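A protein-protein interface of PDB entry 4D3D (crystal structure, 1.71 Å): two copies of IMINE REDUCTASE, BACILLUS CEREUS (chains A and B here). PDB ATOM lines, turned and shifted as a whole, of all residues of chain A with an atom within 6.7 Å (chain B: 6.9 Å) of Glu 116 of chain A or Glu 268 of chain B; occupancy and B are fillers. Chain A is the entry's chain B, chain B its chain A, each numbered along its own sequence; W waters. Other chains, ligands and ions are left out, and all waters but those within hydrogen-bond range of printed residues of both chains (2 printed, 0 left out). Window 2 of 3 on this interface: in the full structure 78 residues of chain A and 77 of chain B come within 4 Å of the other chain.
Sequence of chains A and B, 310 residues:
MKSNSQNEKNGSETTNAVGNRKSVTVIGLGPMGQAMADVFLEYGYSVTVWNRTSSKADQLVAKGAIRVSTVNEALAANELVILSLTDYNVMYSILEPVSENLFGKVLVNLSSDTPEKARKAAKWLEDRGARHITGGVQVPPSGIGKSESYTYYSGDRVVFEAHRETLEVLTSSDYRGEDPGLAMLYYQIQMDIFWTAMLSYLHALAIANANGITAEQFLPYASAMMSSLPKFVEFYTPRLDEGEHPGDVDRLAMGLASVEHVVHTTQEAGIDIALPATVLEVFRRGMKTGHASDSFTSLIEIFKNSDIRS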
ATOM      1  N   ASP A 113     -21.220  33.669 -11.991  1.00  0.00           N
ATOM      2  CA  ASP A 113     -21.266  32.257 -11.961  1.00  0.00           C
ATOM      3  C   ASP A 113     -21.324  31.814 -10.489  1.00  0.00           C
ATOM      4  O   ASP A 113     -21.681  32.640  -9.591  1.00  0.00           O
ATOM      5  CB  ASP A 113     -20.039  31.629 -12.735  1.00  0.00           C
ATOM      6  CG  ASP A 113     -20.373  30.286 -13.383  1.00  0.00           C
ATOM      7  OD1 ASP A 113     -21.005  29.310 -12.814  1.00  0.00           O
ATOM      8  OD2 ASP A 113     -19.967  30.112 -14.551  1.00  0.00           O
ATOM      9  N   THR A 114     -21.159  30.517 -10.310  1.00  0.00           N
ATOM     10  CA  THR A 114     -21.308  29.889  -9.072  1.00  0.00           C
ATOM     11  C   THR A 114     -20.045  30.213  -8.195  1.00  0.00           C
ATOM     12  O   THR A 114     -18.939  30.567  -8.687  1.00  0.00           O
ATOM     13  CB  THR A 114     -21.503  28.406  -9.190  1.00  0.00           C
ATOM     14  OG1 THR A 114     -20.294  27.715  -9.571  1.00  0.00           O
ATOM     15  CG2 THR A 114     -22.678  28.033 -10.171  1.00  0.00           C
ATOM     16  N   PRO A 115     -20.207  29.984  -6.899  1.00  0.00           N
ATOM     17  CA  PRO A 115     -19.053  30.082  -5.992  1.00  0.00           C
ATOM     18  C   PRO A 115     -17.956  29.078  -6.393  1.00  0.00           C
ATOM     19  O   PRO A 115     -16.785  29.423  -6.338  1.00  0.00           O
ATOM     20  CB  PRO A 115     -19.688  29.698  -4.656  1.00  0.00           C
ATOM     21  CG  PRO A 115     -21.125  30.214  -4.758  1.00  0.00           C
ATOM     22  CD  PRO A 115     -21.507  29.876  -6.166  1.00  0.00           C
ATOM     23  N   GLU A 116     -18.315  27.848  -6.760  1.00  0.00           N
ATOM     24  CA  GLU A 116     -17.294  26.827  -7.078  1.00  0.00           C
ATOM     25  C   GLU A 116     -16.514  27.206  -8.337  1.00  0.00           C
ATOM     26  O   GLU A 116     -15.298  27.001  -8.409  1.00  0.00           O
ATOM     27  CB  GLU A 116     -17.894  25.457  -7.187  1.00  0.00           C
ATOM     28  CG  GLU A 116     -16.954  24.348  -7.674  1.00  0.00           C
ATOM     29  CD  GLU A 116     -17.602  22.948  -7.826  1.00  0.00           C
ATOM     30  OE1 GLU A 116     -18.790  22.739  -7.472  1.00  0.00           O
ATOM     31  OE2 GLU A 116     -16.881  21.992  -8.251  1.00  0.00           O
ATOM     32  N   LYS A 117     -17.157  27.817  -9.290  1.00  0.00           N
ATOM     33  CA  LYS A 117     -16.417  28.254 -10.502  1.00  0.00           C
ATOM     34  C   LYS A 117     -15.326  29.331 -10.183  1.00  0.00           C
ATOM     35  O   LYS A 117     -14.202  29.228 -10.672  1.00  0.00           O
ATOM     36  CB  LYS A 117     -17.396  28.728 -11.552  1.00  0.00           C
ATOM     37  CG  LYS A 117     -18.192  27.506 -12.124  1.00  0.00           C
ATOM     38  CD  LYS A 117     -18.295  27.417 -13.647  1.00  0.00           C
ATOM     39  CE  LYS A 117     -16.961  27.648 -14.350  1.00  0.00           C
ATOM     40  NZ  LYS A 117     -16.674  26.910 -15.642  1.00  0.00           N
ATOM     41  N   ALA A 118     -15.643  30.284  -9.309  1.00  0.00           N
ATOM     42  CA  ALA A 118     -14.733  31.273  -8.826  1.00  0.00           C
ATOM     43  C   ALA A 118     -13.588  30.639  -8.017  1.00  0.00           C
ATOM     44  O   ALA A 118     -12.430  31.035  -8.194  1.00  0.00           O
ATOM     45  CB  ALA A 118     -15.424  32.303  -7.987  1.00  0.00           C
ATOM     46  N   ARG A 119     -13.897  29.673  -7.158  1.00  0.00           N
ATOM     47  CA  ARG A 119     -12.844  28.973  -6.422  1.00  0.00           C
ATOM     48  C   ARG A 119     -11.884  28.232  -7.363  1.00  0.00           C
ATOM     49  O   ARG A 119     -10.661  28.267  -7.125  1.00  0.00           O
ATOM     50  CB  ARG A 119     -13.448  27.983  -5.453  1.00  0.00           C
ATOM     51  CG  ARG A 119     -14.219  28.645  -4.288  1.00  0.00           C
ATOM     52  CD  ARG A 119     -15.119  27.650  -3.538  1.00  0.00           C
ATOM     53  NE  ARG A 119     -15.877  28.376  -2.482  1.00  0.00           N
ATOM     54  CZ  ARG A 119     -17.153  28.077  -2.147  1.00  0.00           C
ATOM     55  NH1 ARG A 119     -17.777  27.085  -2.724  1.00  0.00           N
ATOM     56  NH2 ARG A 119     -17.829  28.820  -1.291  1.00  0.00           N
ATOM     57  N   LYS A 120     -12.423  27.522  -8.343  1.00  0.00           N
ATOM     58  CA  LYS A 120     -11.579  26.727  -9.234  1.00  0.00           C
ATOM     59  C   LYS A 120     -10.685  27.663 -10.061  1.00  0.00           C
ATOM     60  O   LYS A 120      -9.471  27.362 -10.229  1.00  0.00           O
ATOM     61  CB  LYS A 120     -12.423  25.867 -10.142  1.00  0.00           C
ATOM     62  CG  LYS A 120     -13.032  24.614  -9.468  1.00  0.00           C
ATOM     63  CD  LYS A 120     -13.707  23.714 -10.488  1.00  0.00           C
ATOM     64  N   ALA A 121     -11.202  28.836 -10.488  1.00  0.00           N
ATOM     65  CA  ALA A 121     -10.404  29.816 -11.188  1.00  0.00           C
ATOM     66  C   ALA A 121      -9.276  30.399 -10.346  1.00  0.00           C
ATOM     67  O   ALA A 121      -8.108  30.522 -10.800  1.00  0.00           O
ATOM     68  CB  ALA A 121     -11.243  30.913 -11.714  1.00  0.00           C
ATOM     69  N   GLY A 181     -15.128  32.162  -3.435  1.00  0.00           N
ATOM     70  CA  GLY A 181     -16.526  31.869  -3.780  1.00  0.00           C
ATOM     71  C   GLY A 181     -17.500  32.885  -3.157  1.00  0.00           C
ATOM     72  O   GLY A 181     -18.641  32.985  -3.613  1.00  0.00           O
ATOM     73  N   MET A 184     -19.569  35.594  -5.153  1.00  0.00           N
ATOM     74  CA  MET A 184     -20.632  34.980  -5.948  1.00  0.00           C
ATOM     75  C   MET A 184     -21.763  34.421  -5.043  1.00  0.00           C
ATOM     76  O   MET A 184     -22.949  34.433  -5.428  1.00  0.00           O
ATOM     77  CB  MET A 184     -20.075  33.894  -6.862  1.00  0.00           C
ATOM     78  CG  MET A 184     -19.107  34.435  -7.976  1.00  0.00           C
ATOM     79  SD  MET A 184     -19.362  36.143  -8.602  1.00  0.00           S
ATOM     80  CE  MET A 184     -20.766  35.485  -9.188  1.00  0.00           C
ATOM     81  N   ALA B 210     -24.487  25.841   3.571  1.00  0.00           N
ATOM     82  CA  ALA B 210     -23.625  24.774   2.964  1.00  0.00           C
ATOM     83  C   ALA B 210     -22.267  25.324   2.652  1.00  0.00           C
ATOM     84  O   ALA B 210     -21.284  24.585   2.664  1.00  0.00           O
ATOM     85  CB  ALA B 210     -24.309  24.221   1.724  1.00  0.00           C
ATOM     86  N   ASN B 211     -22.177  26.614   2.358  1.00  0.00           N
ATOM     87  CA  ASN B 211     -20.930  27.320   1.944  1.00  0.00           C
ATOM     88  C   ASN B 211     -20.188  27.935   3.131  1.00  0.00           C
ATOM     89  O   ASN B 211     -19.174  28.663   2.961  1.00  0.00           O
ATOM     90  CB  ASN B 211     -21.236  28.430   0.914  1.00  0.00           C
ATOM     91  CG  ASN B 211     -21.416  27.873  -0.488  1.00  0.00           C
ATOM     92  OD1 ASN B 211     -20.439  27.792  -1.260  1.00  0.00           O
ATOM     93  ND2 ASN B 211     -22.645  27.464  -0.845  1.00  0.00           N
ATOM     94  N   VAL B 263     -29.927  28.196 -10.034  1.00  0.00           N
ATOM     95  CA  VAL B 263     -30.073  26.773 -10.096  1.00  0.00           C
ATOM     96  C   VAL B 263     -28.724  26.031  -9.960  1.00  0.00           C
ATOM     97  O   VAL B 263     -28.599  25.093  -9.170  1.00  0.00           O
ATOM     98  CB  VAL B 263     -30.856  26.323 -11.375  1.00  0.00           C
ATOM     99  CG1 VAL B 263     -30.859  24.814 -11.512  1.00  0.00           C
ATOM    100  CG2 VAL B 263     -32.311  26.785 -11.297  1.00  0.00           C
ATOM    101  N   HIS B 264     -27.724  26.417 -10.741  1.00  0.00           N
ATOM    102  CA  HIS B 264     -26.443  25.780 -10.653  1.00  0.00           C
ATOM    103  C   HIS B 264     -25.784  25.952  -9.255  1.00  0.00           C
ATOM    104  O   HIS B 264     -25.167  25.005  -8.729  1.00  0.00           O
ATOM    105  CB  HIS B 264     -25.489  26.326 -11.681  1.00  0.00           C
ATOM    106  CG  HIS B 264     -25.920  26.047 -13.087  1.00  0.00           C
ATOM    107  ND1 HIS B 264     -25.531  26.844 -14.149  1.00  0.00           N
ATOM    108  CD2 HIS B 264     -26.779  25.128 -13.582  1.00  0.00           C
ATOM    109  CE1 HIS B 264     -26.146  26.418 -15.247  1.00  0.00           C
ATOM    110  NE2 HIS B 264     -26.877  25.359 -14.943  1.00  0.00           N
ATOM    111  N   THR B 265     -25.936  27.123  -8.670  1.00  0.00           N
ATOM    112  CA  THR B 265     -25.415  27.425  -7.312  1.00  0.00           C
ATOM    113  C   THR B 265     -26.066  26.490  -6.288  1.00  0.00           C
ATOM    114  O   THR B 265     -25.385  25.919  -5.388  1.00  0.00           O
ATOM    115  CB  THR B 265     -25.658  28.892  -6.967  1.00  0.00           C
ATOM    116  OG1 THR B 265     -24.932  29.775  -7.848  1.00  0.00           O
ATOM    117  CG2 THR B 265     -25.247  29.235  -5.518  1.00  0.00           C
ATOM    118  N   THR B 266     -27.387  26.270  -6.478  1.00  0.00           N
ATOM    119  CA  THR B 266     -28.189  25.372  -5.643  1.00  0.00           C
ATOM    120  C   THR B 266     -27.644  23.951  -5.727  1.00  0.00           C
ATOM    121  O   THR B 266     -27.402  23.304  -4.719  1.00  0.00           O
ATOM    122  CB  THR B 266     -29.691  25.402  -5.982  1.00  0.00           C
ATOM    123  OG1 THR B 266     -30.162  26.746  -5.906  1.00  0.00           O
ATOM    124  CG2 THR B 266     -30.488  24.559  -5.012  1.00  0.00           C
ATOM    125  N   GLN B 267     -27.423  23.473  -6.959  1.00  0.00           N
ATOM    126  CA  GLN B 267     -26.969  22.098  -7.139  1.00  0.00           C
ATOM    127  C   GLN B 267     -25.584  21.870  -6.574  1.00  0.00           C
ATOM    128  O   GLN B 267     -25.339  20.800  -6.001  1.00  0.00           O
ATOM    129  CB  GLN B 267     -26.968  21.765  -8.660  1.00  0.00           C
ATOM    130  CG  GLN B 267     -28.282  21.658  -9.345  1.00  0.00           C
ATOM    131  CD  GLN B 267     -28.178  21.667 -10.856  1.00  0.00           C
ATOM    132  OE1 GLN B 267     -27.392  22.383 -11.456  1.00  0.00           O
ATOM    133  NE2 GLN B 267     -28.996  20.838 -11.463  1.00  0.00           N
ATOM    134  N   GLU B 268     -24.709  22.825  -6.773  1.00  0.00           N
ATOM    135  CA  GLU B 268     -23.303  22.759  -6.306  1.00  0.00           C
ATOM    136  C   GLU B 268     -23.282  22.674  -4.772  1.00  0.00           C
ATOM    137  O   GLU B 268     -22.386  22.031  -4.209  1.00  0.00           O
ATOM    138  CB  GLU B 268     -22.482  23.970  -6.710  1.00  0.00           C
ATOM    139  CG  GLU B 268     -22.062  24.023  -8.155  1.00  0.00           C
ATOM    140  CD  GLU B 268     -21.232  25.291  -8.414  1.00  0.00           C
ATOM    141  OE1 GLU B 268     -20.966  26.150  -7.468  1.00  0.00           O
ATOM    142  OE2 GLU B 268     -20.981  25.469  -9.602  1.00  0.00           O
ATOM    143  N   ALA B 269     -24.259  23.332  -4.113  1.00  0.00           N
ATOM    144  CA  ALA B 269     -24.349  23.330  -2.642  1.00  0.00           C
ATOM    145  C   ALA B 269     -25.031  22.096  -2.080  1.00  0.00           C
ATOM    146  O   ALA B 269     -25.154  21.961  -0.837  1.00  0.00           O
ATOM    147  CB  ALA B 269     -25.052  24.596  -2.156  1.00  0.00           C
ATOM    148  N   GLY B 270     -25.478  21.174  -2.925  1.00  0.00           N
ATOM    149  CA  GLY B 270     -26.260  20.024  -2.532  1.00  0.00           C
ATOM    150  C   GLY B 270     -27.648  20.315  -1.952  1.00  0.00           C
ATOM    151  O   GLY B 270     -28.196  19.509  -1.206  1.00  0.00           O
ATOM    152  N   ILE B 271     -28.227  21.422  -2.341  1.00  0.00           N
ATOM    153  CA  ILE B 271     -29.543  21.872  -1.811  1.00  0.00           C
ATOM    154  C   ILE B 271     -30.673  21.433  -2.735  1.00  0.00           C
ATOM    155  O   ILE B 271     -30.485  21.310  -3.964  1.00  0.00           O
ATOM    156  CB  ILE B 271     -29.452  23.385  -1.531  1.00  0.00           C
ATOM    157  CG1 ILE B 271     -28.402  23.738  -0.454  1.00  0.00           C
ATOM    158  CG2 ILE B 271     -30.833  24.045  -1.204  1.00  0.00           C
ATOM    159  CD1 ILE B 271     -28.463  22.900   0.805  1.00  0.00           C
ATOM    160  N   ILE B 273     -33.487  21.228  -5.267  1.00  0.00           N
ATOM    161  CA  ILE B 273     -33.652  22.017  -6.465  1.00  0.00           C
ATOM    162  C   ILE B 273     -35.144  22.427  -6.788  1.00  0.00           C
ATOM    163  O   ILE B 273     -35.364  23.293  -7.676  1.00  0.00           O
ATOM    164  CB  ILE B 273     -33.120  21.194  -7.654  1.00  0.00           C
ATOM    165  CG1 ILE B 273     -32.666  22.118  -8.666  1.00  0.00           C
ATOM    166  CG2 ILE B 273     -34.102  20.124  -8.185  1.00  0.00           C
ATOM    167  CD1 ILE B 273     -31.347  22.645  -8.241  1.00  0.00           C
HETATM  168  O   HOH W   1     -19.977  21.119  -4.940  1.00  0.00           O
HETATM  169  O   HOH W   2     -23.831  28.952 -13.812  1.00  0.00           O
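Of the printed residues of chain B, Thr 114 of chain A touches His 264 (3.6 Å), Thr 265 (3.7 Å) and Glu 268 (2.3 Å). Glu 116 of chain A touches one residue of chain B. Printed residues of chain B within 4 Å of Arg 119 of chain A: Asn 211. Printed residues of chain A within 4 Å of Asn 211 of chain B: Pro 115 and Arg 119. Of the printed residues of chain A, His 264 of chain B touches Thr 114 (3.6 Å). Printed residues of chain A within 4 Å of Thr 265 of chain B: Thr 114 and Pro 115. Of chain A, only Thr 114, Pro 115 and Glu 116 come within 4 Å of Glu 268 of chain B. The nearest residue of chain B that does not touch Glu 116 of chain A is Asn 211 of chain B (5.9 Å).
OD1 of Asn 211 of chain B is in hydrogen-bond range of NH2 of Arg 119 of chain A (2.8 Å). The side-chain carboxylate (OE1) of Glu 268 of chain B is in hydrogen-bond range of the side-chain hydroxyl (OG1) of Thr 114 of chain A (2.7 Å). OE1 of Glu 268 of chain B sits close to N of Glu 116 of chain A.
No position is printed for both chains. Of the 8 pairs that touch across the chains among the printed residues, none has its exchanged pair printed and touching as well.
Among the printed residues, merely in contact across the chains: Thr 114 of chain A with His 264 of chain B, Thr 114 of chain A with Thr 265 of chain B, Pro 115 of chain A with Asn 211 of chain B, Pro 115 of chain A with Thr 265 of chain B and Pro 115 of chain A with Glu 268 of chain B.
OG1 of Thr 114 of chain A sits close to N of Glu 116 of chain A, 3.4 Å away. N of Lys 117 of chain A sits at hydrogen-bond distance from OG1 of Thr 114 of chain A (3.2 Å).
Of the 11 printed residues of chain A, 4 touch a printed residue of chain B. Along chain A the printed residues that touch a printed residue of chain B span positions 114 to 119. Of the 12 printed residues of chain B, 4 touch a printed residue of chain A. Hydrophobic or aromatic side chains of chain B within 4 Å of the printed part of chain A: His 264. Among the printed residues, 8 pairs touch across the chains. Among the printed residues, no Asp or Glu carboxylate lies within 4 Å of a Lys or Arg side-chain nitrogen of the other chain.
Water W1 lies within hydrogen-bond range of the backbone carbonyl oxygen (O) of Glu 268 of chain B (2.7 Å) and the side-chain carboxylate (OE1) of Glu 116 of chain A (3.2 Å). Water W2 bridges ND1 of His 264 of chain B (2.7 Å) and OD1 of Asp 113 of chain A (3.0 Å).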
